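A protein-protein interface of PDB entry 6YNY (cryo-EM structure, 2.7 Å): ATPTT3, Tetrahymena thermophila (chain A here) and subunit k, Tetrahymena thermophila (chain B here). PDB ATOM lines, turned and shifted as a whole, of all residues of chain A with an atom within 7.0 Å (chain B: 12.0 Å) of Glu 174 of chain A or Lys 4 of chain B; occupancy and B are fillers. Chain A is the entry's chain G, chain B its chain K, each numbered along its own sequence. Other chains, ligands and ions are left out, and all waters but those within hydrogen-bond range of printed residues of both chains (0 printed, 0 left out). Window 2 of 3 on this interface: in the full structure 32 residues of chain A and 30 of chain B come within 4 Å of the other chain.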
ATOM      1  N   ARG A 158      16.304  28.007  18.366  1.00  0.00           N
ATOM      2  CA  ARG A 158      15.628  28.089  19.654  1.00  0.00           C
ATOM      3  C   ARG A 158      16.616  28.322  20.786  1.00  0.00           C
ATOM      4  O   ARG A 158      16.295  29.017  21.757  1.00  0.00           O
ATOM      5  CB  ARG A 158      14.814  26.823  19.898  1.00  0.00           C
ATOM      6  CG  ARG A 158      13.682  26.643  18.911  1.00  0.00           C
ATOM      7  CD  ARG A 158      12.625  25.706  19.432  1.00  0.00           C
ATOM      8  NE  ARG A 158      11.487  25.623  18.528  1.00  0.00           N
ATOM      9  CZ  ARG A 158      10.327  25.059  18.838  1.00  0.00           C
ATOM     10  NH1 ARG A 158      10.137  24.530  20.037  1.00  0.00           N
ATOM     11  NH2 ARG A 158       9.350  25.031  17.947  1.00  0.00           N
ATOM     12  N   TYR A 162      16.146  31.690  23.182  1.00  0.00           N
ATOM     13  CA  TYR A 162      15.991  31.431  24.606  1.00  0.00           C
ATOM     14  C   TYR A 162      17.171  31.937  25.420  1.00  0.00           C
ATOM     15  O   TYR A 162      17.128  31.867  26.652  1.00  0.00           O
ATOM     16  CB  TYR A 162      15.791  29.937  24.849  1.00  0.00           C
ATOM     17  CG  TYR A 162      14.523  29.373  24.247  1.00  0.00           C
ATOM     18  CD1 TYR A 162      13.426  30.182  23.993  1.00  0.00           C
ATOM     19  CD2 TYR A 162      14.425  28.028  23.933  1.00  0.00           C
ATOM     20  CE1 TYR A 162      12.275  29.670  23.446  1.00  0.00           C
ATOM     21  CE2 TYR A 162      13.276  27.508  23.384  1.00  0.00           C
ATOM     22  CZ  TYR A 162      12.205  28.333  23.142  1.00  0.00           C
ATOM     23  OH  TYR A 162      11.058  27.815  22.593  1.00  0.00           O
ATOM     24  N   PHE A 171       8.302  34.250  26.597  1.00  0.00           N
ATOM     25  CA  PHE A 171       8.249  32.971  25.908  1.00  0.00           C
ATOM     26  C   PHE A 171       9.115  31.945  26.619  1.00  0.00           C
ATOM     27  O   PHE A 171      10.213  32.256  27.086  1.00  0.00           O
ATOM     28  CB  PHE A 171       8.706  33.114  24.459  1.00  0.00           C
ATOM     29  CG  PHE A 171       7.805  33.973  23.630  1.00  0.00           C
ATOM     30  CD1 PHE A 171       6.799  33.411  22.872  1.00  0.00           C
ATOM     31  CD2 PHE A 171       7.960  35.343  23.614  1.00  0.00           C
ATOM     32  CE1 PHE A 171       5.970  34.200  22.114  1.00  0.00           C
ATOM     33  CE2 PHE A 171       7.132  36.133  22.858  1.00  0.00           C
ATOM     34  CZ  PHE A 171       6.137  35.561  22.108  1.00  0.00           C
ATOM     35  N   ASN A 172       8.609  30.718  26.693  1.00  0.00           N
ATOM     36  CA  ASN A 172       9.340  29.593  27.246  1.00  0.00           C
ATOM     37  C   ASN A 172       8.973  28.349  26.453  1.00  0.00           C
ATOM     38  O   ASN A 172       7.854  28.225  25.949  1.00  0.00           O
ATOM     39  CB  ASN A 172       9.033  29.393  28.733  1.00  0.00           C
ATOM     40  CG  ASN A 172       9.817  28.253  29.341  1.00  0.00           C
ATOM     41  OD1 ASN A 172       9.327  27.129  29.441  1.00  0.00           O
ATOM     42  ND2 ASN A 172      11.046  28.535  29.750  1.00  0.00           N
ATOM     43  N   GLU A 173       9.929  27.428  26.344  1.00  0.00           N
ATOM     44  CA  GLU A 173       9.721  26.253  25.507  1.00  0.00           C
ATOM     45  C   GLU A 173       8.547  25.417  25.989  1.00  0.00           C
ATOM     46  O   GLU A 173       7.839  24.814  25.175  1.00  0.00           O
ATOM     47  CB  GLU A 173      10.994  25.410  25.469  1.00  0.00           C
ATOM     48  CG  GLU A 173      10.919  24.195  24.563  1.00  0.00           C
ATOM     49  CD  GLU A 173      10.393  24.520  23.178  1.00  0.00           C
ATOM     50  OE1 GLU A 173       9.165  24.428  22.972  1.00  0.00           O
ATOM     51  OE2 GLU A 173      11.200  24.880  22.297  1.00  0.00           O
ATOM     52  N   GLU A 174       8.316  25.371  27.297  1.00  0.00           N
ATOM     53  CA  GLU A 174       7.214  24.600  27.852  1.00  0.00           C
ATOM     54  C   GLU A 174       5.865  25.277  27.662  1.00  0.00           C
ATOM     55  O   GLU A 174       4.844  24.703  28.057  1.00  0.00           O
ATOM     56  CB  GLU A 174       7.454  24.343  29.339  1.00  0.00           C
ATOM     57  CG  GLU A 174       8.715  23.559  29.630  1.00  0.00           C
ATOM     58  CD  GLU A 174       8.853  23.192  31.091  1.00  0.00           C
ATOM     59  OE1 GLU A 174       7.904  23.449  31.860  1.00  0.00           O
ATOM     60  OE2 GLU A 174       9.910  22.648  31.471  1.00  0.00           O
ATOM     61  N   THR A 175       5.833  26.472  27.070  1.00  0.00           N
ATOM     62  CA  THR A 175       4.585  27.204  26.909  1.00  0.00           C
ATOM     63  C   THR A 175       4.453  27.846  25.534  1.00  0.00           C
ATOM     64  O   THR A 175       3.518  28.627  25.323  1.00  0.00           O
ATOM     65  CB  THR A 175       4.463  28.286  27.986  1.00  0.00           C
ATOM     66  OG1 THR A 175       5.582  29.175  27.904  1.00  0.00           O
ATOM     67  CG2 THR A 175       4.423  27.662  29.360  1.00  0.00           C
ATOM     68  N   ILE A 176       5.341  27.543  24.601  1.00  0.00           N
ATOM     69  CA  ILE A 176       5.339  28.152  23.279  1.00  0.00           C
ATOM     70  C   ILE A 176       4.665  27.211  22.294  1.00  0.00           C
ATOM     71  O   ILE A 176       4.745  25.984  22.415  1.00  0.00           O
ATOM     72  CB  ILE A 176       6.774  28.491  22.830  1.00  0.00           C
ATOM     73  CG1 ILE A 176       6.754  29.361  21.582  1.00  0.00           C
ATOM     74  CG2 ILE A 176       7.549  27.235  22.542  1.00  0.00           C
ATOM     75  CD1 ILE A 176       8.116  29.793  21.147  1.00  0.00           C
ATOM     76  N   ASP A 221       2.567  32.192  23.205  1.00  0.00           N
ATOM     77  CA  ASP A 221       2.855  31.679  24.537  1.00  0.00           C
ATOM     78  C   ASP A 221       1.547  31.536  25.298  1.00  0.00           C
ATOM     79  O   ASP A 221       0.847  32.526  25.531  1.00  0.00           O
ATOM     80  CB  ASP A 221       3.819  32.596  25.285  1.00  0.00           C
ATOM     81  CG  ASP A 221       4.277  32.005  26.601  1.00  0.00           C
ATOM     82  OD1 ASP A 221       4.992  30.982  26.576  1.00  0.00           O
ATOM     83  OD2 ASP A 221       3.924  32.561  27.661  1.00  0.00           O
ATOM     84  N   VAL A 222       1.224  30.302  25.689  1.00  0.00           N
ATOM     85  CA  VAL A 222      -0.038  30.026  26.362  1.00  0.00           C
ATOM     86  C   VAL A 222      -0.076  30.537  27.792  1.00  0.00           C
ATOM     87  O   VAL A 222      -1.149  30.547  28.404  1.00  0.00           O
ATOM     88  CB  VAL A 222      -0.330  28.511  26.343  1.00  0.00           C
ATOM     89  CG1 VAL A 222      -0.443  28.017  24.921  1.00  0.00           C
ATOM     90  CG2 VAL A 222       0.749  27.737  27.084  1.00  0.00           C
ATOM     91  N   MET B   1       6.970  21.480  23.268  1.00  0.00           N
ATOM     92  CA  MET B   1       8.150  21.370  24.161  1.00  0.00           C
ATOM     93  C   MET B   1       9.089  20.271  23.690  1.00  0.00           C
ATOM     94  O   MET B   1       9.766  19.639  24.496  1.00  0.00           O
ATOM     95  CB  MET B   1       7.709  21.096  25.597  1.00  0.00           C
ATOM     96  CG  MET B   1       6.866  19.854  25.766  1.00  0.00           C
ATOM     97  SD  MET B   1       6.741  19.351  27.490  1.00  0.00           S
ATOM     98  CE  MET B   1       6.216  20.884  28.244  1.00  0.00           C
ATOM     99  N   TRP B   2       9.129  20.043  22.378  1.00  0.00           N
ATOM    100  CA  TRP B   2      10.004  19.004  21.851  1.00  0.00           C
ATOM    101  C   TRP B   2      11.470  19.370  22.020  1.00  0.00           C
ATOM    102  O   TRP B   2      12.313  18.482  22.182  1.00  0.00           O
ATOM    103  CB  TRP B   2       9.682  18.741  20.383  1.00  0.00           C
ATOM    104  CG  TRP B   2       9.931  19.891  19.483  1.00  0.00           C
ATOM    105  CD1 TRP B   2       9.036  20.840  19.104  1.00  0.00           C
ATOM    106  CD2 TRP B   2      11.161  20.217  18.835  1.00  0.00           C
ATOM    107  NE1 TRP B   2       9.632  21.741  18.261  1.00  0.00           N
ATOM    108  CE2 TRP B   2      10.938  21.378  18.079  1.00  0.00           C
ATOM    109  CE3 TRP B   2      12.431  19.638  18.822  1.00  0.00           C
ATOM    110  CZ2 TRP B   2      11.936  21.973  17.322  1.00  0.00           C
ATOM    111  CZ3 TRP B   2      13.416  20.227  18.070  1.00  0.00           C
ATOM    112  CH2 TRP B   2      13.166  21.384  17.330  1.00  0.00           C
ATOM    113  N   TYR B   3      11.794  20.663  21.993  1.00  0.00           N
ATOM    114  CA  TYR B   3      13.165  21.094  22.227  1.00  0.00           C
ATOM    115  C   TYR B   3      13.605  20.828  23.658  1.00  0.00           C
ATOM    116  O   TYR B   3      14.808  20.705  23.911  1.00  0.00           O
ATOM    117  CB  TYR B   3      13.295  22.577  21.891  1.00  0.00           C
ATOM    118  CG  TYR B   3      14.664  23.159  22.132  1.00  0.00           C
ATOM    119  CD1 TYR B   3      15.696  22.953  21.231  1.00  0.00           C
ATOM    120  CD2 TYR B   3      14.920  23.929  23.252  1.00  0.00           C
ATOM    121  CE1 TYR B   3      16.946  23.487  21.448  1.00  0.00           C
ATOM    122  CE2 TYR B   3      16.165  24.467  23.476  1.00  0.00           C
ATOM    123  CZ  TYR B   3      17.174  24.245  22.572  1.00  0.00           C
ATOM    124  OH  TYR B   3      18.416  24.784  22.796  1.00  0.00           O
ATOM    125  N   LYS B   4      12.660  20.729  24.593  1.00  0.00           N
ATOM    126  CA  LYS B   4      13.006  20.393  25.968  1.00  0.00           C
ATOM    127  C   LYS B   4      13.607  18.999  26.057  1.00  0.00           C
ATOM    128  O   LYS B   4      14.527  18.759  26.846  1.00  0.00           O
ATOM    129  CB  LYS B   4      11.763  20.492  26.848  1.00  0.00           C
ATOM    130  CG  LYS B   4      11.946  20.004  28.266  1.00  0.00           C
ATOM    131  CD  LYS B   4      10.640  20.065  29.022  1.00  0.00           C
ATOM    132  CE  LYS B   4      10.781  19.535  30.429  1.00  0.00           C
ATOM    133  NZ  LYS B   4       9.481  19.562  31.149  1.00  0.00           N
ATOM    134  N   TYR B   5      13.096  18.069  25.261  1.00  0.00           N
ATOM    135  CA  TYR B   5      13.563  16.692  25.271  1.00  0.00           C
ATOM    136  C   TYR B   5      14.624  16.420  24.218  1.00  0.00           C
ATOM    137  O   TYR B   5      15.127  15.295  24.143  1.00  0.00           O
ATOM    138  CB  TYR B   5      12.380  15.744  25.082  1.00  0.00           C
ATOM    139  CG  TYR B   5      11.329  15.890  26.153  1.00  0.00           C
ATOM    140  CD1 TYR B   5      11.591  15.511  27.458  1.00  0.00           C
ATOM    141  CD2 TYR B   5      10.077  16.403  25.862  1.00  0.00           C
ATOM    142  CE1 TYR B   5      10.641  15.640  28.441  1.00  0.00           C
ATOM    143  CE2 TYR B   5       9.119  16.537  26.840  1.00  0.00           C
ATOM    144  CZ  TYR B   5       9.407  16.152  28.129  1.00  0.00           C
ATOM    145  OH  TYR B   5       8.461  16.279  29.117  1.00  0.00           O
ATOM    146  N   PHE B   6      14.972  17.413  23.408  1.00  0.00           N
ATOM    147  CA  PHE B   6      16.061  17.260  22.458  1.00  0.00           C
ATOM    148  C   PHE B   6      17.394  17.256  23.194  1.00  0.00           C
ATOM    149  O   PHE B   6      17.648  18.111  24.047  1.00  0.00           O
ATOM    150  CB  PHE B   6      16.020  18.385  21.428  1.00  0.00           C
ATOM    151  CG  PHE B   6      17.252  18.483  20.586  1.00  0.00           C
ATOM    152  CD1 PHE B   6      17.411  17.682  19.475  1.00  0.00           C
ATOM    153  CD2 PHE B   6      18.249  19.381  20.903  1.00  0.00           C
ATOM    154  CE1 PHE B   6      18.543  17.771  18.703  1.00  0.00           C
ATOM    155  CE2 PHE B   6      19.380  19.473  20.135  1.00  0.00           C
ATOM    156  CZ  PHE B   6      19.528  18.668  19.033  1.00  0.00           C
ATOM    157  N   SER B   7      18.239  16.285  22.868  1.00  0.00           N
ATOM    158  CA  SER B   7      19.538  16.135  23.506  1.00  0.00           C
ATOM    159  C   SER B   7      20.593  16.851  22.673  1.00  0.00           C
ATOM    160  O   SER B   7      20.776  16.537  21.493  1.00  0.00           O
ATOM    161  CB  SER B   7      19.892  14.660  23.669  1.00  0.00           C
ATOM    162  OG  SER B   7      21.069  14.506  24.435  1.00  0.00           O
ATOM    163  N   LYS B   8      21.284  17.809  23.288  1.00  0.00           N
ATOM    164  CA  LYS B   8      22.299  18.574  22.580  1.00  0.00           C
ATOM    165  C   LYS B   8      23.559  17.770  22.300  1.00  0.00           C
ATOM    166  O   LYS B   8      24.440  18.268  21.591  1.00  0.00           O
ATOM    167  CB  LYS B   8      22.658  19.822  23.380  1.00  0.00           C
ATOM    168  CG  LYS B   8      21.521  20.795  23.521  1.00  0.00           C
ATOM    169  CD  LYS B   8      21.932  21.999  24.322  1.00  0.00           C
ATOM    170  CE  LYS B   8      20.902  23.099  24.231  1.00  0.00           C
ATOM    171  NZ  LYS B   8      19.562  22.646  24.663  1.00  0.00           N
ATOM    172  N   GLN B   9      23.673  16.555  22.829  1.00  0.00           N
ATOM    173  CA  GLN B   9      24.842  15.742  22.534  1.00  0.00           C
ATOM    174  C   GLN B   9      24.856  15.253  21.095  1.00  0.00           C
ATOM    175  O   GLN B   9      25.831  14.617  20.682  1.00  0.00           O
ATOM    176  CB  GLN B   9      24.917  14.557  23.501  1.00  0.00           C
ATOM    177  CG  GLN B   9      23.908  13.473  23.248  1.00  0.00           C
ATOM    178  CD  GLN B   9      23.900  12.418  24.335  1.00  0.00           C
ATOM    179  OE1 GLN B   9      24.032  11.226  24.063  1.00  0.00           O
ATOM    180  NE2 GLN B   9      23.736  12.851  25.575  1.00  0.00           N
ATOM    181  N   SER B  10      23.800  15.529  20.330  1.00  0.00           N
ATOM    182  CA  SER B  10      23.782  15.247  18.905  1.00  0.00           C
ATOM    183  C   SER B  10      24.413  16.358  18.081  1.00  0.00           C
ATOM    184  O   SER B  10      24.553  16.201  16.863  1.00  0.00           O
ATOM    185  CB  SER B  10      22.347  15.020  18.436  1.00  0.00           C
ATOM    186  OG  SER B  10      21.538  16.145  18.709  1.00  0.00           O
ATOM    187  N   TRP B  11      24.791  17.469  18.707  1.00  0.00           N
ATOM    188  CA  TRP B  11      25.480  18.550  18.020  1.00  0.00           C
ATOM    189  C   TRP B  11      26.946  18.247  17.763  1.00  0.00           C
ATOM    190  O   TRP B  11      27.654  19.107  17.230  1.00  0.00           O
ATOM    191  CB  TRP B  11      25.364  19.841  18.829  1.00  0.00           C
ATOM    192  CG  TRP B  11      24.011  20.459  18.811  1.00  0.00           C
ATOM    193  CD1 TRP B  11      22.960  20.109  18.022  1.00  0.00           C
ATOM    194  CD2 TRP B  11      23.559  21.544  19.622  1.00  0.00           C
ATOM    195  NE1 TRP B  11      21.881  20.909  18.291  1.00  0.00           N
ATOM    196  CE2 TRP B  11      22.224  21.798  19.272  1.00  0.00           C
ATOM    197  CE3 TRP B  11      24.155  22.323  20.615  1.00  0.00           C
ATOM    198  CZ2 TRP B  11      21.476  22.797  19.876  1.00  0.00           C
ATOM    199  CZ3 TRP B  11      23.411  23.313  21.211  1.00  0.00           C
ATOM    200  CH2 TRP B  11      22.086  23.543  20.840  1.00  0.00           C
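The side-chain hydroxyl of Tyr 3 of chain B is in hydrogen-bond range of the side-chain amino group of Lys 8 of chain B (3.1 Å).
The guanidinium group of Arg 158 of chain A is in salt-bridge range of the side-chain carboxylate of Glu 173 of chain A (2.5 Å).
The side-chain hydroxyl (OH) of Tyr 162 of chain A lies within hydrogen-bond range of the side-chain carboxylate (OE2) of Glu 173 of chain A (3.0 Å).
The side-chain amide oxygen (OD1) of Asn 172 of chain A lies within hydrogen-bond range of the backbone NH (N) of Glu 174 of chain A (3.0 Å).
Lys 4 of chain B touches just these residues of chain A: Glu 173 and Glu 174.
No residue of chain B comes within 4 Å of Asn 172 of chain A.
Printed residues of chain B within 4 Å of Glu 173 of chain A: Met 1, Tyr 3 and Lys 4.
No residue of chain B comes within 4 Å of Ile 176 of chain A.
Of the printed residues of chain A, Trp 2 of chain B touches Arg 158 (3.3 Å).
Of the printed residues of chain B, Arg 158 of chain A touches Trp 2.
Printed residues of chain A within 4 Å of Met 1 of chain B: Glu 173 and Glu 174.
The nearest printed residue of chain A that does not touch Trp 2 of chain B is Glu 173 of chain A (4.4 Å).
The side-chain amino group (NZ) of Lys 4 of chain B lies within salt-bridge range of the side-chain carboxylate (OE2) of Glu 174 of chain A (3.1 Å).
The guanidinium group (NH2) of Arg 158 of chain A lies close to the indole nitrogen (NE1) of Trp 2 of chain B (3.3 Å).
Of the 11 printed residues of chain B, 4 touch a printed residue of chain A.
Printed residues of chain B that touch a printed residue of chain A: Met 1, Trp 2, Tyr 3 and Lys 4.
Hydrophobic or aromatic side chains of chain B that line the printed part of chain A: Met 1, Trp 2 and Tyr 3.
Along chain B the printed residues that touch a printed residue of chain A span positions 1 to 4.
Hydrophobic or aromatic side chains of chain A that line the printed part of chain B: Tyr 162.
Among the printed residues, 7 pairs touch across the chains.
Among the printed residues, Asp or Glu carboxylates within 4 Å of a Lys or Arg side-chain nitrogen of the other chain: Glu 174 of chain A with Lys 4 of chain B.
Among the printed residues, pairs that only touch across the chains: Tyr 162 of chain A with Tyr 3 of chain B, Glu 173 of chain A with Met 1 of chain B, Glu 173 of chain A with Tyr 3 of chain B, Glu 173 of chain A with Lys 4 of chain B and Glu 174 of chain A with Met 1 of chain B.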
